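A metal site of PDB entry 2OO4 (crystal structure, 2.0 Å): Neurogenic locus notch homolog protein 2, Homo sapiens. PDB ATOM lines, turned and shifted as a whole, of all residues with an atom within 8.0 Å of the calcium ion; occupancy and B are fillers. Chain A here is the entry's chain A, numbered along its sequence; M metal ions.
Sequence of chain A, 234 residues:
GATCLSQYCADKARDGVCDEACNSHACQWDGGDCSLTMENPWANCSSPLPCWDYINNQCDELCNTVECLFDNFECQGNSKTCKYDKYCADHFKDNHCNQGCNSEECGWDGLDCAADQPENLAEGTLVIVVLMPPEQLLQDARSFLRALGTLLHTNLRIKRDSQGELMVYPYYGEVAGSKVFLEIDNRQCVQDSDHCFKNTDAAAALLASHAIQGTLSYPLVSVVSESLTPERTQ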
ATOM      1  N   TYR A   8     -20.281  22.430 -15.454  1.00  0.00           N
ATOM      2  CA  TYR A   8     -21.684  22.190 -15.084  1.00  0.00           C
ATOM      3  C   TYR A   8     -22.632  22.805 -16.096  1.00  0.00           C
ATOM      4  O   TYR A   8     -23.644  22.213 -16.459  1.00  0.00           O
ATOM      5  CB  TYR A   8     -21.980  22.767 -13.694  1.00  0.00           C
ATOM      6  CG  TYR A   8     -23.422  22.642 -13.255  1.00  0.00           C
ATOM      7  CD1 TYR A   8     -23.954  21.409 -12.856  1.00  0.00           C
ATOM      8  CD2 TYR A   8     -24.259  23.761 -13.221  1.00  0.00           C
ATOM      9  CE1 TYR A   8     -25.280  21.299 -12.447  1.00  0.00           C
ATOM     10  CE2 TYR A   8     -25.596  23.655 -12.820  1.00  0.00           C
ATOM     11  CZ  TYR A   8     -26.085  22.424 -12.431  1.00  0.00           C
ATOM     12  OH  TYR A   8     -27.398  22.311 -12.028  1.00  0.00           O
ATOM     13  N   CYS A   9     -22.287  24.011 -16.538  1.00  0.00           N
ATOM     14  CA  CYS A   9     -23.095  24.756 -17.498  1.00  0.00           C
ATOM     15  C   CYS A   9     -23.001  24.182 -18.906  1.00  0.00           C
ATOM     16  O   CYS A   9     -23.973  24.241 -19.658  1.00  0.00           O
ATOM     17  CB  CYS A   9     -22.735  26.238 -17.457  1.00  0.00           C
ATOM     18  SG  CYS A   9     -23.309  27.034 -15.936  1.00  0.00           S
ATOM     19  N   ALA A  10     -21.850  23.600 -19.239  1.00  0.00           N
ATOM     20  CA  ALA A  10     -21.705  22.887 -20.511  1.00  0.00           C
ATOM     21  C   ALA A  10     -22.704  21.741 -20.575  1.00  0.00           C
ATOM     22  O   ALA A  10     -23.373  21.537 -21.599  1.00  0.00           O
ATOM     23  CB  ALA A  10     -20.271  22.387 -20.698  1.00  0.00           C
ATOM     24  N   ASP A  11     -22.821  21.013 -19.466  1.00  0.00           N
ATOM     25  CA  ASP A  11     -23.684  19.832 -19.357  1.00  0.00           C
ATOM     26  C   ASP A  11     -25.161  20.198 -19.429  1.00  0.00           C
ATOM     27  O   ASP A  11     -25.970  19.433 -19.961  1.00  0.00           O
ATOM     28  CB  ASP A  11     -23.397  19.088 -18.046  1.00  0.00           C
ATOM     29  CG  ASP A  11     -23.907  17.654 -18.052  1.00  0.00           C
ATOM     30  OD1 ASP A  11     -23.071  16.724 -18.018  1.00  0.00           O
ATOM     31  OD2 ASP A  11     -25.148  17.451 -18.077  1.00  0.00           O
ATOM     32  N   LYS A  12     -25.511  21.371 -18.896  1.00  0.00           N
ATOM     33  CA  LYS A  12     -26.907  21.743 -18.730  1.00  0.00           C
ATOM     34  C   LYS A  12     -27.476  22.558 -19.893  1.00  0.00           C
ATOM     35  O   LYS A  12     -28.690  22.685 -20.022  1.00  0.00           O
ATOM     36  CB  LYS A  12     -27.108  22.467 -17.397  1.00  0.00           C
ATOM     37  CG  LYS A  12     -27.059  21.554 -16.175  1.00  0.00           C
ATOM     38  CD  LYS A  12     -28.344  20.756 -15.998  1.00  0.00           C
ATOM     39  CE  LYS A  12     -28.240  19.710 -14.904  1.00  0.00           C
ATOM     40  NZ  LYS A  12     -27.618  18.452 -15.407  1.00  0.00           N
ATOM     41  N   ALA A  13     -26.595  23.099 -20.725  1.00  0.00           N
ATOM     42  CA  ALA A  13     -27.012  23.950 -21.840  1.00  0.00           C
ATOM     43  C   ALA A  13     -28.004  23.254 -22.761  1.00  0.00           C
ATOM     44  O   ALA A  13     -27.854  22.078 -23.084  1.00  0.00           O
ATOM     45  CB  ALA A  13     -25.793  24.420 -22.612  1.00  0.00           C
ATOM     46  N   ARG A  14     -29.039  23.989 -23.163  1.00  0.00           N
ATOM     47  CA  ARG A  14     -29.992  23.560 -24.187  1.00  0.00           C
ATOM     48  C   ARG A  14     -30.622  22.189 -23.895  1.00  0.00           C
ATOM     49  O   ARG A  14     -30.702  21.316 -24.773  1.00  0.00           O
ATOM     50  CB  ARG A  14     -29.302  23.555 -25.555  1.00  0.00           C
ATOM     51  CG  ARG A  14     -30.185  23.931 -26.729  1.00  0.00           C
ATOM     52  CD  ARG A  14     -29.351  24.172 -27.985  1.00  0.00           C
ATOM     53  NE  ARG A  14     -28.381  25.267 -27.815  1.00  0.00           N
ATOM     54  CZ  ARG A  14     -27.079  25.103 -27.612  1.00  0.00           C
ATOM     55  NH1 ARG A  14     -26.544  23.885 -27.538  1.00  0.00           N
ATOM     56  NH2 ARG A  14     -26.293  26.156 -27.473  1.00  0.00           N
ATOM     57  N   ASP A  15     -31.052  21.991 -22.651  1.00  0.00           N
ATOM     58  CA  ASP A  15     -31.694  20.733 -22.252  1.00  0.00           C
ATOM     59  C   ASP A  15     -33.195  20.875 -21.984  1.00  0.00           C
ATOM     60  O   ASP A  15     -33.853  19.926 -21.558  1.00  0.00           O
ATOM     61  CB  ASP A  15     -30.952  20.085 -21.064  1.00  0.00           C
ATOM     62  CG  ASP A  15     -31.193  20.802 -19.729  1.00  0.00           C
ATOM     63  OD1 ASP A  15     -31.457  22.025 -19.697  1.00  0.00           O
ATOM     64  OD2 ASP A  15     -31.088  20.109 -18.687  1.00  0.00           O
ATOM     65  N   GLY A  16     -33.726  22.068 -22.247  1.00  0.00           N
ATOM     66  CA  GLY A  16     -35.144  22.348 -22.074  1.00  0.00           C
ATOM     67  C   GLY A  16     -35.527  22.772 -20.670  1.00  0.00           C
ATOM     68  O   GLY A  16     -36.715  22.888 -20.361  1.00  0.00           O
ATOM     69  N   VAL A  17     -34.530  22.991 -19.813  1.00  0.00           N
ATOM     70  CA  VAL A  17     -34.768  23.440 -18.436  1.00  0.00           C
ATOM     71  C   VAL A  17     -33.849  24.614 -18.110  1.00  0.00           C
ATOM     72  O   VAL A  17     -32.644  24.543 -18.354  1.00  0.00           O
ATOM     73  CB  VAL A  17     -34.532  22.292 -17.421  1.00  0.00           C
ATOM     74  CG1 VAL A  17     -34.618  22.796 -15.970  1.00  0.00           C
ATOM     75  CG2 VAL A  17     -35.518  21.144 -17.649  1.00  0.00           C
ATOM     76  N   CYS A  18     -34.424  25.697 -17.575  1.00  0.00           N
ATOM     77  CA  CYS A  18     -33.620  26.836 -17.100  1.00  0.00           C
ATOM     78  C   CYS A  18     -32.904  26.484 -15.789  1.00  0.00           C
ATOM     79  O   CYS A  18     -33.538  26.196 -14.770  1.00  0.00           O
ATOM     80  CB  CYS A  18     -34.494  28.087 -16.916  1.00  0.00           C
ATOM     81  SG  CYS A  18     -33.585  29.588 -16.418  1.00  0.00           S
ATOM     82  N   ASP A  19     -31.573  26.523 -15.841  1.00  0.00           N
ATOM     83  CA  ASP A  19     -30.710  26.331 -14.680  1.00  0.00           C
ATOM     84  C   ASP A  19     -30.060  27.653 -14.325  1.00  0.00           C
ATOM     85  O   ASP A  19     -29.197  28.148 -15.063  1.00  0.00           O
ATOM     86  CB  ASP A  19     -29.653  25.282 -14.992  1.00  0.00           C
ATOM     87  CG  ASP A  19     -30.253  23.950 -15.372  1.00  0.00           C
ATOM     88  OD1 ASP A  19     -30.843  23.291 -14.493  1.00  0.00           O
ATOM     89  OD2 ASP A  19     -30.147  23.554 -16.555  1.00  0.00           O
ATOM     90  N   GLU A  20     -30.458  28.226 -13.182  1.00  0.00           N
ATOM     91  CA  GLU A  20     -30.152  29.621 -12.850  1.00  0.00           C
ATOM     92  C   GLU A  20     -28.662  29.878 -12.607  1.00  0.00           C
ATOM     93  O   GLU A  20     -28.193  31.010 -12.761  1.00  0.00           O
ATOM     94  CB  GLU A  20     -31.014  30.134 -11.681  1.00  0.00           C
ATOM     95  CG  GLU A  20     -32.517  30.282 -12.007  1.00  0.00           C
ATOM     96  CD  GLU A  20     -32.849  31.515 -12.862  1.00  0.00           C
ATOM     97  OE1 GLU A  20     -32.032  32.451 -12.951  1.00  0.00           O
ATOM     98  OE2 GLU A  20     -33.964  31.543 -13.439  1.00  0.00           O
ATOM     99  N   CYS A  22     -26.540  28.955 -14.534  1.00  0.00           N
ATOM    100  CA  CYS A  22     -26.034  29.161 -15.883  1.00  0.00           C
ATOM    101  C   CYS A  22     -26.805  30.252 -16.613  1.00  0.00           C
ATOM    102  O   CYS A  22     -26.593  30.471 -17.803  1.00  0.00           O
ATOM    103  CB  CYS A  22     -26.126  27.860 -16.669  1.00  0.00           C
ATOM    104  SG  CYS A  22     -25.271  26.506 -15.880  1.00  0.00           S
ATOM    105  N   TRP A  29     -27.430  32.465 -21.472  1.00  0.00           N
ATOM    106  CA  TRP A  29     -28.621  32.176 -20.665  1.00  0.00           C
ATOM    107  C   TRP A  29     -29.034  30.709 -20.673  1.00  0.00           C
ATOM    108  O   TRP A  29     -30.155  30.336 -21.047  1.00  0.00           O
ATOM    109  CB  TRP A  29     -29.768  33.184 -20.963  1.00  0.00           C
ATOM    110  CG  TRP A  29     -29.309  34.546 -20.491  1.00  0.00           C
ATOM    111  CD1 TRP A  29     -29.224  34.984 -19.184  1.00  0.00           C
ATOM    112  CD2 TRP A  29     -28.754  35.578 -21.295  1.00  0.00           C
ATOM    113  NE1 TRP A  29     -28.693  36.256 -19.141  1.00  0.00           N
ATOM    114  CE2 TRP A  29     -28.396  36.636 -20.430  1.00  0.00           C
ATOM    115  CE3 TRP A  29     -28.531  35.721 -22.673  1.00  0.00           C
ATOM    116  CZ2 TRP A  29     -27.838  37.824 -20.890  1.00  0.00           C
ATOM    117  CZ3 TRP A  29     -27.981  36.897 -23.128  1.00  0.00           C
ATOM    118  CH2 TRP A  29     -27.630  37.936 -22.238  1.00  0.00           C
ATOM    119  N   ASP A  30     -28.090  29.885 -20.242  1.00  0.00           N
ATOM    120  CA  ASP A  30     -28.228  28.430 -20.186  1.00  0.00           C
ATOM    121  C   ASP A  30     -28.505  27.807 -21.565  1.00  0.00           C
ATOM    122  O   ASP A  30     -29.431  27.008 -21.726  1.00  0.00           O
ATOM    123  CB  ASP A  30     -29.280  28.047 -19.149  1.00  0.00           C
ATOM    124  CG  ASP A  30     -29.298  26.572 -18.833  1.00  0.00           C
ATOM    125  OD1 ASP A  30     -30.328  26.099 -18.323  1.00  0.00           O
ATOM    126  OD2 ASP A  30     -28.287  25.872 -19.095  1.00  0.00           O
ATOM    127  N   GLY A  31     -27.693  28.180 -22.547  1.00  0.00           N
ATOM    128  CA  GLY A  31     -27.900  27.758 -23.943  1.00  0.00           C
ATOM    129  C   GLY A  31     -29.291  28.075 -24.493  1.00  0.00           C
ATOM    130  O   GLY A  31     -29.813  27.356 -25.350  1.00  0.00           O
ATOM    131  N   GLY A  32     -29.892  29.151 -23.991  1.00  0.00           N
ATOM    132  CA  GLY A  32     -31.225  29.591 -24.425  1.00  0.00           C
ATOM    133  C   GLY A  32     -32.381  28.999 -23.642  1.00  0.00           C
ATOM    134  O   GLY A  32     -33.540  29.376 -23.868  1.00  0.00           O
ATOM    135  N   ASP A  33     -32.083  28.079 -22.719  1.00  0.00           N
ATOM    136  CA  ASP A  33     -33.131  27.491 -21.882  1.00  0.00           C
ATOM    137  C   ASP A  33     -33.903  28.525 -21.050  1.00  0.00           C
ATOM    138  O   ASP A  33     -35.082  28.341 -20.737  1.00  0.00           O
ATOM    139  CB  ASP A  33     -32.556  26.422 -20.960  1.00  0.00           C
ATOM    140  CG  ASP A  33     -32.090  25.192 -21.704  1.00  0.00           C
ATOM    141  OD1 ASP A  33     -32.615  24.882 -22.800  1.00  0.00           O
ATOM    142  OD2 ASP A  33     -31.173  24.531 -21.181  1.00  0.00           O
ATOM    143  N   CYS A  34     -33.227  29.632 -20.721  1.00  0.00           N
ATOM    144  CA  CYS A  34     -33.803  30.675 -19.869  1.00  0.00           C
ATOM    145  C   CYS A  34     -34.267  31.892 -20.660  1.00  0.00           C
ATOM    146  O   CYS A  34     -34.809  32.831 -20.085  1.00  0.00           O
ATOM    147  CB  CYS A  34     -32.759  31.132 -18.869  1.00  0.00           C
ATOM    148  SG  CYS A  34     -32.140  29.824 -17.817  1.00  0.00           S
HETATM  149 CA    CA M   1     -30.425  24.025 -18.970  1.00  0.00          CA
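Of the 20 residues printed, 6 come within 4 Å of the calcium ion. The nearest printed residue that does not touch the calcium ion is Ala 13 (4.3 Å).
The calcium ion is bound by the side-chain carboxylate (OD1) of Asp 30 (2.2 Å), the backbone carbonyl oxygen (O) of Val 17 (2.4 Å), the side-chain carboxylate (OD1) of Asp 15 (2.4 Å), the side-chain carboxylate (OD2) of Asp 33 (2.4 Å), the backbone carbonyl oxygen (O) of Lys 12 (2.4 Å), the side-chain carboxylate (OD2) of Asp 19 (2.5 Å) and the side-chain carboxylate (OD2) of Asp 30 (2.8 Å).
O of Asp 30 lies within hydrogen-bond range of N of Arg 14, 3.4 Å away. The backbone NH of Asp 30 is in hydrogen-bond range of the backbone carbonyl oxygen of Cys 22 (2.9 Å). The backbone NH (N) of Arg 14 lies close to the side-chain carboxylate (OD2) of Asp 33, at 3.0 Å. OD1 of Asp 33 sits at hydrogen-bond distance from N of Gly 16, at 3.1 Å. The side-chain amino group of Lys 12 is in salt-bridge range of the side-chain carboxylate of Asp 11, at 3.8 Å. The side-chain sulfur (SG) of Cys 34 forms a disulfide with the side-chain sulfur (SG) of Cys 18, at 2.0 Å. SG of Cys 22 is disulfide-bonded to SG of Cys 9 (2.0 Å).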
